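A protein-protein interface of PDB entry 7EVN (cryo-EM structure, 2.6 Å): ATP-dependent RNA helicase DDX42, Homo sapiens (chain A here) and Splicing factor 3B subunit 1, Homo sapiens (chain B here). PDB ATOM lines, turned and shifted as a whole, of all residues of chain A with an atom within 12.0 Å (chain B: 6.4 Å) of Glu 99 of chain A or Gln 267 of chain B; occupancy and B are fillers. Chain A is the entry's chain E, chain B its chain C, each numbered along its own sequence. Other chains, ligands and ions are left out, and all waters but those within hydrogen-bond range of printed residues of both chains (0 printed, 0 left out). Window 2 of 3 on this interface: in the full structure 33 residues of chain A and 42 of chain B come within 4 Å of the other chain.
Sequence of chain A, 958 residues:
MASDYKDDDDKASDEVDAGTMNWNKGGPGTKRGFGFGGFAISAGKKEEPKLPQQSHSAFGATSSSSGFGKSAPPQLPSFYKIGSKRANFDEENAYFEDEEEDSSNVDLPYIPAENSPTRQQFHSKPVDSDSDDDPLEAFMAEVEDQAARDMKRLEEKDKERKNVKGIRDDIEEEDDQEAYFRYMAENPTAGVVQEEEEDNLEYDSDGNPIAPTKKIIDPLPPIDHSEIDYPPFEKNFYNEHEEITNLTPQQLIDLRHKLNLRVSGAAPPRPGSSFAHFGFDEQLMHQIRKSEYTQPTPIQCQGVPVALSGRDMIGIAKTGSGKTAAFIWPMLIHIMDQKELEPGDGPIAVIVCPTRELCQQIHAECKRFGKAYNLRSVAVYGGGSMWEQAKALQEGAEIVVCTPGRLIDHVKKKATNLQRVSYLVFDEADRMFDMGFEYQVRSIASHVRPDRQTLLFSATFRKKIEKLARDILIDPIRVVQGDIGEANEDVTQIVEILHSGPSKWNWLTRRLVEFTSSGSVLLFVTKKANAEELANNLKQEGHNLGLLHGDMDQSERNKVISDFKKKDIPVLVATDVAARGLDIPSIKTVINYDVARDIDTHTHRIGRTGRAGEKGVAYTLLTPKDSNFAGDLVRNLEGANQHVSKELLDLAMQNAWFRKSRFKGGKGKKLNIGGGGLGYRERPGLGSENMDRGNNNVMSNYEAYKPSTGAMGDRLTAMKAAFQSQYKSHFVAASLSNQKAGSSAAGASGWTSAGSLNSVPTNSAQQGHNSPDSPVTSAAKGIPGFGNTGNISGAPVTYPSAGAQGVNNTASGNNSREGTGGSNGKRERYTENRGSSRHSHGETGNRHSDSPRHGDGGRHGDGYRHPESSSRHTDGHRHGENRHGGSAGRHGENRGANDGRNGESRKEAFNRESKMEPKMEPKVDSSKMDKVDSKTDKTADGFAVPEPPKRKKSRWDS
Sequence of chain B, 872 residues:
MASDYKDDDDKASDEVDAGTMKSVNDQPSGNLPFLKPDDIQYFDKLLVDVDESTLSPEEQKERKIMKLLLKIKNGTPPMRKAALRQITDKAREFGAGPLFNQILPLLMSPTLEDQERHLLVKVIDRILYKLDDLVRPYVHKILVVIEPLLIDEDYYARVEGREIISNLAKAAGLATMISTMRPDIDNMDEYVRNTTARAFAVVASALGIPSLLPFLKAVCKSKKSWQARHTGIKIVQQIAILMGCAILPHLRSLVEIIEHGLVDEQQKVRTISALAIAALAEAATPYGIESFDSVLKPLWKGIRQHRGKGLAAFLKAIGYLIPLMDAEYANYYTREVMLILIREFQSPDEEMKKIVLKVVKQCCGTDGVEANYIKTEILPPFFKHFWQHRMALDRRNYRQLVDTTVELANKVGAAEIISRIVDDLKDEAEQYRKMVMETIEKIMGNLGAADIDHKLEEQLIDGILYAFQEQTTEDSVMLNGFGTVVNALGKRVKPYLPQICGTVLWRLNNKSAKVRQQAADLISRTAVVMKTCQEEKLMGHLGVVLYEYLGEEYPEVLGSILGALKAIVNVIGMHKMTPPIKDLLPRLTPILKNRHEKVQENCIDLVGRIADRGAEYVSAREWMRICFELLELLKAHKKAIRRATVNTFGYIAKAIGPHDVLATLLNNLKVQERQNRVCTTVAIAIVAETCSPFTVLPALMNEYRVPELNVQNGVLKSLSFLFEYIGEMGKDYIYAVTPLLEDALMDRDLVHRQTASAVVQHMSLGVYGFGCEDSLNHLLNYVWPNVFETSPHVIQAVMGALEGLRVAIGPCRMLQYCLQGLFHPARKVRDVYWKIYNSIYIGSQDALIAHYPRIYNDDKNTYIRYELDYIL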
ATOM      1  N   GLU A  91     -30.642  27.237  10.380  1.00  0.00           N
ATOM      2  CA  GLU A  91     -31.594  26.093  10.363  1.00  0.00           C
ATOM      3  C   GLU A  91     -31.359  25.258   9.097  1.00  0.00           C
ATOM      4  O   GLU A  91     -31.791  24.090   9.066  1.00  0.00           O
ATOM      5  CB  GLU A  91     -33.031  26.588  10.532  1.00  0.00           C
ATOM      6  CG  GLU A  91     -33.183  27.570  11.681  1.00  0.00           C
ATOM      7  CD  GLU A  91     -34.545  27.587  12.358  1.00  0.00           C
ATOM      8  OE1 GLU A  91     -35.243  26.556  12.303  1.00  0.00           O
ATOM      9  OE2 GLU A  91     -34.901  28.631  12.940  1.00  0.00           O
ATOM     10  N   GLU A  92     -30.700  25.859   8.101  1.00  0.00           N
ATOM     11  CA  GLU A  92     -30.354  25.214   6.806  1.00  0.00           C
ATOM     12  C   GLU A  92     -29.124  24.328   7.020  1.00  0.00           C
ATOM     13  O   GLU A  92     -29.125  23.185   6.527  1.00  0.00           O
ATOM     14  CB  GLU A  92     -30.032  26.278   5.754  1.00  0.00           C
ATOM     15  CG  GLU A  92     -31.260  26.912   5.129  1.00  0.00           C
ATOM     16  CD  GLU A  92     -30.987  27.667   3.838  1.00  0.00           C
ATOM     17  OE1 GLU A  92     -29.823  27.674   3.396  1.00  0.00           O
ATOM     18  OE2 GLU A  92     -31.940  28.246   3.278  1.00  0.00           O
ATOM     19  N   ASN A  93     -28.146  24.827   7.780  1.00  0.00           N
ATOM     20  CA  ASN A  93     -26.902  24.057   8.042  1.00  0.00           C
ATOM     21  C   ASN A  93     -27.270  22.765   8.777  1.00  0.00           C
ATOM     22  O   ASN A  93     -26.783  21.705   8.364  1.00  0.00           O
ATOM     23  CB  ASN A  93     -25.904  24.872   8.867  1.00  0.00           C
ATOM     24  CG  ASN A  93     -25.597  26.223   8.258  1.00  0.00           C
ATOM     25  OD1 ASN A  93     -25.875  26.458   7.085  1.00  0.00           O
ATOM     26  ND2 ASN A  93     -25.023  27.116   9.047  1.00  0.00           N
ATOM     27  N   ALA A  94     -28.157  22.853   9.772  1.00  0.00           N
ATOM     28  CA  ALA A  94     -28.570  21.664  10.554  1.00  0.00           C
ATOM     29  C   ALA A  94     -29.269  20.661   9.630  1.00  0.00           C
ATOM     30  O   ALA A  94     -28.964  19.449   9.716  1.00  0.00           O
ATOM     31  CB  ALA A  94     -29.480  22.094  11.677  1.00  0.00           C
ATOM     32  N   TYR A  95     -30.104  21.173   8.718  1.00  0.00           N
ATOM     33  CA  TYR A  95     -30.871  20.339   7.750  1.00  0.00           C
ATOM     34  C   TYR A  95     -29.923  19.586   6.814  1.00  0.00           C
ATOM     35  O   TYR A  95     -30.132  18.381   6.601  1.00  0.00           O
ATOM     36  CB  TYR A  95     -31.810  21.216   6.918  1.00  0.00           C
ATOM     37  CG  TYR A  95     -32.435  20.524   5.731  1.00  0.00           C
ATOM     38  CD1 TYR A  95     -33.014  19.271   5.852  1.00  0.00           C
ATOM     39  CD2 TYR A  95     -32.461  21.129   4.484  1.00  0.00           C
ATOM     40  CE1 TYR A  95     -33.595  18.633   4.770  1.00  0.00           C
ATOM     41  CE2 TYR A  95     -33.037  20.504   3.391  1.00  0.00           C
ATOM     42  CZ  TYR A  95     -33.606  19.253   3.534  1.00  0.00           C
ATOM     43  OH  TYR A  95     -34.176  18.634   2.460  1.00  0.00           O
ATOM     44  N   PHE A  96     -28.929  20.285   6.257  1.00  0.00           N
ATOM     45  CA  PHE A  96     -27.962  19.653   5.319  1.00  0.00           C
ATOM     46  C   PHE A  96     -27.044  18.696   6.086  1.00  0.00           C
ATOM     47  O   PHE A  96     -26.875  17.544   5.647  1.00  0.00           O
ATOM     48  CB  PHE A  96     -27.195  20.721   4.537  1.00  0.00           C
ATOM     49  CG  PHE A  96     -27.943  21.256   3.344  1.00  0.00           C
ATOM     50  CD1 PHE A  96     -28.443  20.398   2.381  1.00  0.00           C
ATOM     51  CD2 PHE A  96     -28.163  22.615   3.193  1.00  0.00           C
ATOM     52  CE1 PHE A  96     -29.140  20.890   1.290  1.00  0.00           C
ATOM     53  CE2 PHE A  96     -28.859  23.105   2.100  1.00  0.00           C
ATOM     54  CZ  PHE A  96     -29.343  22.241   1.150  1.00  0.00           C
ATOM     55  N   GLU A  97     -26.483  19.159   7.205  1.00  0.00           N
ATOM     56  CA  GLU A  97     -25.589  18.316   8.043  1.00  0.00           C
ATOM     57  C   GLU A  97     -26.453  17.460   8.974  1.00  0.00           C
ATOM     58  O   GLU A  97     -26.489  17.748  10.184  1.00  0.00           O
ATOM     59  CB  GLU A  97     -24.629  19.196   8.848  1.00  0.00           C
ATOM     60  CG  GLU A  97     -23.241  19.284   8.244  1.00  0.00           C
ATOM     61  CD  GLU A  97     -22.330  18.109   8.562  1.00  0.00           C
ATOM     62  OE1 GLU A  97     -22.376  17.108   7.821  1.00  0.00           O
ATOM     63  OE2 GLU A  97     -21.573  18.202   9.548  1.00  0.00           O
ATOM     64  N   ASP A  98     -27.117  16.441   8.416  1.00  0.00           N
ATOM     65  CA  ASP A  98     -28.011  15.545   9.191  1.00  0.00           C
ATOM     66  C   ASP A  98     -28.125  14.209   8.449  1.00  0.00           C
ATOM     67  O   ASP A  98     -28.222  13.166   9.122  1.00  0.00           O
ATOM     68  CB  ASP A  98     -29.382  16.191   9.399  1.00  0.00           C
ATOM     69  CG  ASP A  98     -30.268  15.438  10.375  1.00  0.00           C
ATOM     70  OD1 ASP A  98     -31.232  16.050  10.881  1.00  0.00           O
ATOM     71  OD2 ASP A  98     -29.989  14.247  10.620  1.00  0.00           O
ATOM     72  N   GLU A  99     -28.118  14.258   7.112  1.00  0.00           N
ATOM     73  CA  GLU A  99     -28.200  13.030   6.278  1.00  0.00           C
ATOM     74  C   GLU A  99     -26.786  12.497   6.038  1.00  0.00           C
ATOM     75  O   GLU A  99     -26.145  12.941   5.069  1.00  0.00           O
ATOM     76  CB  GLU A  99     -28.903  13.312   4.950  1.00  0.00           C
ATOM     77  CG  GLU A  99     -30.135  12.454   4.730  1.00  0.00           C
ATOM     78  CD  GLU A  99     -29.849  11.066   4.189  1.00  0.00           C
ATOM     79  OE1 GLU A  99     -28.752  10.543   4.458  1.00  0.00           O
ATOM     80  OE2 GLU A  99     -30.724  10.512   3.497  1.00  0.00           O
ATOM     81  N   GLU A 100     -26.285  11.619   6.932  1.00  0.00           N
ATOM     82  CA  GLU A 100     -24.906  11.020   6.881  1.00  0.00           C
ATOM     83  C   GLU A 100     -24.960   9.532   7.284  1.00  0.00           C
ATOM     84  O   GLU A 100     -25.771   9.208   8.173  1.00  0.00           O
ATOM     85  CB  GLU A 100     -23.952  11.800   7.787  1.00  0.00           C
ATOM     86  CG  GLU A 100     -22.519  11.816   7.284  1.00  0.00           C
ATOM     87  CD  GLU A 100     -21.555  12.608   8.149  1.00  0.00           C
ATOM     88  OE1 GLU A 100     -21.035  12.035   9.127  1.00  0.00           O
ATOM     89  OE2 GLU A 100     -21.326  13.794   7.844  1.00  0.00           O
ATOM     90  N   GLU A 101     -24.137   8.654   6.663  1.00  0.00           N
ATOM     91  CA  GLU A 101     -24.192   7.181   6.827  1.00  0.00           C
ATOM     92  C   GLU A 101     -22.782   6.594   6.695  1.00  0.00           C
ATOM     93  O   GLU A 101     -22.251   6.645   5.568  1.00  0.00           O
ATOM     94  CB  GLU A 101     -25.133   6.553   5.799  1.00  0.00           C
ATOM     95  CG  GLU A 101     -26.599   6.902   6.004  1.00  0.00           C
ATOM     96  CD  GLU A 101     -27.491   6.321   4.923  1.00  0.00           C
ATOM     97  OE1 GLU A 101     -26.954   5.811   3.918  1.00  0.00           O
ATOM     98  OE2 GLU A 101     -28.729   6.377   5.079  1.00  0.00           O
ATOM     99  N   ASP B 264     -19.881  12.606  -7.645  1.00  0.00           N
ATOM    100  CA  ASP B 264     -19.385  11.570  -6.760  1.00  0.00           C
ATOM    101  C   ASP B 264     -20.479  10.539  -6.500  1.00  0.00           C
ATOM    102  O   ASP B 264     -21.671  10.814  -6.625  1.00  0.00           O
ATOM    103  CB  ASP B 264     -18.902  12.194  -5.451  1.00  0.00           C
ATOM    104  CG  ASP B 264     -18.008  11.270  -4.654  1.00  0.00           C
ATOM    105  OD1 ASP B 264     -18.529  10.315  -4.042  1.00  0.00           O
ATOM    106  OD2 ASP B 264     -16.782  11.494  -4.640  1.00  0.00           O
ATOM    107  N   GLU B 265     -20.060   9.329  -6.142  1.00  0.00           N
ATOM    108  CA  GLU B 265     -21.037   8.305  -5.801  1.00  0.00           C
ATOM    109  C   GLU B 265     -21.517   8.415  -4.362  1.00  0.00           C
ATOM    110  O   GLU B 265     -22.386   7.641  -3.947  1.00  0.00           O
ATOM    111  CB  GLU B 265     -20.467   6.908  -6.058  1.00  0.00           C
ATOM    112  CG  GLU B 265     -19.378   6.478  -5.100  1.00  0.00           C
ATOM    113  CD  GLU B 265     -17.998   6.917  -5.548  1.00  0.00           C
ATOM    114  OE1 GLU B 265     -17.903   7.722  -6.498  1.00  0.00           O
ATOM    115  OE2 GLU B 265     -17.005   6.452  -4.950  1.00  0.00           O
ATOM    116  N   GLN B 266     -20.974   9.352  -3.594  1.00  0.00           N
ATOM    117  CA  GLN B 266     -21.447   9.593  -2.238  1.00  0.00           C
ATOM    118  C   GLN B 266     -22.362  10.811  -2.217  1.00  0.00           C
ATOM    119  O   GLN B 266     -21.980  11.899  -2.667  1.00  0.00           O
ATOM    120  CB  GLN B 266     -20.272   9.784  -1.285  1.00  0.00           C
ATOM    121  CG  GLN B 266     -19.807   8.500  -0.643  1.00  0.00           C
ATOM    122  CD  GLN B 266     -20.835   7.923   0.301  1.00  0.00           C
ATOM    123  OE1 GLN B 266     -21.621   8.653   0.903  1.00  0.00           O
ATOM    124  NE2 GLN B 266     -20.828   6.607   0.445  1.00  0.00           N
ATOM    125  N   GLN B 267     -23.566  10.625  -1.677  1.00  0.00           N
ATOM    126  CA  GLN B 267     -24.555  11.695  -1.677  1.00  0.00           C
ATOM    127  C   GLN B 267     -24.130  12.849  -0.779  1.00  0.00           C
ATOM    128  O   GLN B 267     -24.377  14.015  -1.101  1.00  0.00           O
ATOM    129  CB  GLN B 267     -25.908  11.138  -1.250  1.00  0.00           C
ATOM    130  CG  GLN B 267     -27.037  12.135  -1.296  1.00  0.00           C
ATOM    131  CD  GLN B 267     -28.072  11.854  -0.240  1.00  0.00           C
ATOM    132  OE1 GLN B 267     -27.768  11.266   0.796  1.00  0.00           O
ATOM    133  NE2 GLN B 267     -29.305  12.272  -0.492  1.00  0.00           N
ATOM    134  N   LYS B 268     -23.442  12.506   0.313  1.00  0.00           N
ATOM    135  CA  LYS B 268     -22.941  13.511   1.284  1.00  0.00           C
ATOM    136  C   LYS B 268     -21.901  14.391   0.583  1.00  0.00           C
ATOM    137  O   LYS B 268     -21.917  15.614   0.811  1.00  0.00           O
ATOM    138  CB  LYS B 268     -22.352  12.797   2.505  1.00  0.00           C
ATOM    139  CG  LYS B 268     -22.909  13.250   3.847  1.00  0.00           C
ATOM    140  CD  LYS B 268     -22.885  14.753   4.026  1.00  0.00           C
ATOM    141  CE  LYS B 268     -23.907  15.256   5.022  1.00  0.00           C
ATOM    142  NZ  LYS B 268     -23.669  14.716   6.381  1.00  0.00           N
ATOM    143  N   VAL B 269     -21.064  13.790  -0.269  1.00  0.00           N
ATOM    144  CA  VAL B 269     -20.039  14.520  -1.006  1.00  0.00           C
ATOM    145  C   VAL B 269     -20.677  15.385  -2.085  1.00  0.00           C
ATOM    146  O   VAL B 269     -20.276  16.538  -2.289  1.00  0.00           O
ATOM    147  CB  VAL B 269     -19.004  13.542  -1.588  1.00  0.00           C
ATOM    148  CG1 VAL B 269     -17.956  14.287  -2.386  1.00  0.00           C
ATOM    149  CG2 VAL B 269     -18.348  12.759  -0.476  1.00  0.00           C
ATOM    150  N   ARG B 270     -21.688  14.855  -2.778  1.00  0.00           N
ATOM    151  CA  ARG B 270     -22.407  15.660  -3.761  1.00  0.00           C
ATOM    152  C   ARG B 270     -23.049  16.885  -3.116  1.00  0.00           C
ATOM    153  O   ARG B 270     -23.002  17.994  -3.669  1.00  0.00           O
ATOM    154  CB  ARG B 270     -23.461  14.805  -4.460  1.00  0.00           C
ATOM    155  CG  ARG B 270     -22.893  13.779  -5.420  1.00  0.00           C
ATOM    156  CD  ARG B 270     -23.892  13.392  -6.496  1.00  0.00           C
ATOM    157  NE  ARG B 270     -25.124  12.853  -5.940  1.00  0.00           N
ATOM    158  CZ  ARG B 270     -25.264  11.612  -5.488  1.00  0.00           C
ATOM    159  NH1 ARG B 270     -24.249  10.769  -5.530  1.00  0.00           N
ATOM    160  NH2 ARG B 270     -26.423  11.214  -4.992  1.00  0.00           N
ATOM    161  N   THR B 271     -23.642  16.707  -1.936  1.00  0.00           N
ATOM    162  CA  THR B 271     -24.319  17.810  -1.266  1.00  0.00           C
ATOM    163  C   THR B 271     -23.334  18.887  -0.824  1.00  0.00           C
ATOM    164  O   THR B 271     -23.582  20.085  -1.026  1.00  0.00           O
ATOM    165  CB  THR B 271     -25.115  17.281  -0.077  1.00  0.00           C
ATOM    166  OG1 THR B 271     -25.865  16.136  -0.484  1.00  0.00           O
ATOM    167  CG2 THR B 271     -26.076  18.329   0.428  1.00  0.00           C
ATOM    168  N   ILE B 272     -22.211  18.489  -0.221  1.00  0.00           N
ATOM    169  CA  ILE B 272     -21.230  19.488   0.178  1.00  0.00           C
ATOM    170  C   ILE B 272     -20.596  20.163  -1.036  1.00  0.00           C
ATOM    171  O   ILE B 272     -20.254  21.347  -0.962  1.00  0.00           O
ATOM    172  CB  ILE B 272     -20.172  18.876   1.122  1.00  0.00           C
ATOM    173  CG1 ILE B 272     -19.425  19.972   1.883  1.00  0.00           C
ATOM    174  CG2 ILE B 272     -19.185  18.018   0.369  1.00  0.00           C
ATOM    175  CD1 ILE B 272     -20.314  20.992   2.549  1.00  0.00           C
ATOM    176  N   ARG B 307     -33.583  13.990  -6.030  1.00  0.00           N
ATOM    177  CA  ARG B 307     -34.738  14.272  -5.184  1.00  0.00           C
ATOM    178  C   ARG B 307     -34.299  14.267  -3.727  1.00  0.00           C
ATOM    179  O   ARG B 307     -33.602  13.344  -3.299  1.00  0.00           O
ATOM    180  CB  ARG B 307     -35.850  13.236  -5.378  1.00  0.00           C
ATOM    181  CG  ARG B 307     -36.641  13.346  -6.665  1.00  0.00           C
ATOM    182  CD  ARG B 307     -37.837  12.421  -6.617  1.00  0.00           C
ATOM    183  NE  ARG B 307     -37.542  11.229  -5.829  1.00  0.00           N
ATOM    184  CZ  ARG B 307     -38.462  10.391  -5.365  1.00  0.00           C
ATOM    185  NH1 ARG B 307     -39.747  10.612  -5.610  1.00  0.00           N
ATOM    186  NH2 ARG B 307     -38.097   9.332  -4.656  1.00  0.00           N
ATOM    187  N   GLY B 308     -34.711  15.284  -2.967  1.00  0.00           N
ATOM    188  CA  GLY B 308     -34.485  15.330  -1.534  1.00  0.00           C
ATOM    189  C   GLY B 308     -33.548  16.467  -1.143  1.00  0.00           C
ATOM    190  O   GLY B 308     -33.565  17.546  -1.747  1.00  0.00           O
ATOM    191  N   LYS B 309     -32.771  16.211  -0.086  1.00  0.00           N
ATOM    192  CA  LYS B 309     -31.783  17.183   0.450  1.00  0.00           C
ATOM    193  C   LYS B 309     -30.810  17.544  -0.675  1.00  0.00           C
ATOM    194  O   LYS B 309     -30.598  18.750  -0.910  1.00  0.00           O
ATOM    195  CB  LYS B 309     -31.029  16.566   1.631  1.00  0.00           C
ATOM    196  CG  LYS B 309     -30.056  17.496   2.342  1.00  0.00           C
ATOM    197  CD  LYS B 309     -29.132  16.775   3.300  1.00  0.00           C
ATOM    198  CE  LYS B 309     -29.863  15.833   4.232  1.00  0.00           C
ATOM    199  NZ  LYS B 309     -30.921  16.531   5.001  1.00  0.00           N
ATOM    200  N   GLY B 310     -30.263  16.529  -1.353  1.00  0.00           N
ATOM    201  CA  GLY B 310     -29.334  16.788  -2.439  1.00  0.00           C
ATOM    202  C   GLY B 310     -29.930  17.707  -3.485  1.00  0.00           C
ATOM    203  O   GLY B 310     -29.263  18.619  -3.982  1.00  0.00           O
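NZ of Lys 268 of chain B is in salt-bridge range of OE1 of Glu 97 of chain A, at 3.1 Å.
NZ of Lys 268 of chain B sits close to O of Glu 99 of chain A (3.3 Å).
OE2 of Glu 100 of chain A lies within salt-bridge range of NZ of Lys 268 of chain B.
The side-chain amino group of Lys 309 of chain B lies within hydrogen-bond range of the backbone carbonyl oxygen of Tyr 95 of chain A (2.6 Å).
O of Gln 267 of chain B sits at hydrogen-bond distance from OG1 of Thr 271 of chain B (2.7 Å).
Phe 96 of chain A touches Lys 268 of chain B (O to CE, 3.8 Å).
Thr 271 of chain B touches Phe 96 of chain A.
CD1 of Phe 96 of chain A touches CG of Lys 309 of chain B, at 3.3 Å.
OE1 of Gln 267 of chain B touches OE1 of Glu 99 of chain A, at 3.9 Å.
CB of Glu 99 of chain A touches CE of Lys 309 of chain B, 2.8 Å away.
Printed residues of chain B within 4 Å of Tyr 95 of chain A: Lys 309 (2.6 Å).
Of the printed residues of chain B, Phe 96 of chain A touches Lys 268, Thr 271 and Lys 309.
Of the printed residues of chain B, Glu 97 of chain A touches Lys 268 (3.1 Å).
Glu 99 of chain A touches just these residues of chain B: Gln 267 (3.9 Å), Lys 268 (3.2 Å) and Lys 309 (2.8 Å).
Of the printed residues of chain B, Glu 100 of chain A touches Lys 268 (2.9 Å).
Glu 265 of chain B touches none of the printed residues of chain A.
No residue of chain A comes within 4 Å of Gln 266 of chain B.
Of the printed residues of chain A, Gln 267 of chain B touches Glu 99.
Lys 268 of chain B touches four residues of chain A.
Arg 307 of chain B touches none of the printed residues of chain A.
Gly 310 of chain B touches none of the printed residues of chain A.
The nearest printed residue of chain A that does not touch Gln 267 of chain B is Glu 100 of chain A (6.3 Å).
Of the 13 printed residues of chain B, 4 touch a printed residue of chain A.
Printed residues of chain B that touch a printed residue of chain A: Gln 267, Lys 268, Thr 271 and Lys 309.
Along chain B the printed residues that touch a printed residue of chain A span positions 267 to 309.
Hydrophobic or aromatic side chains of chain A within 4 Å of the printed part of chain B: Tyr 95 and Phe 96.
Among the printed residues, 9 pairs touch across the chains.
Among the printed residues, Asp or Glu carboxylates within 4 Å of a Lys or Arg side-chain nitrogen of the other chain: Glu 97 of chain A with Lys 268 of chain B and Glu 100 of chain A with Lys 268 of chain B.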
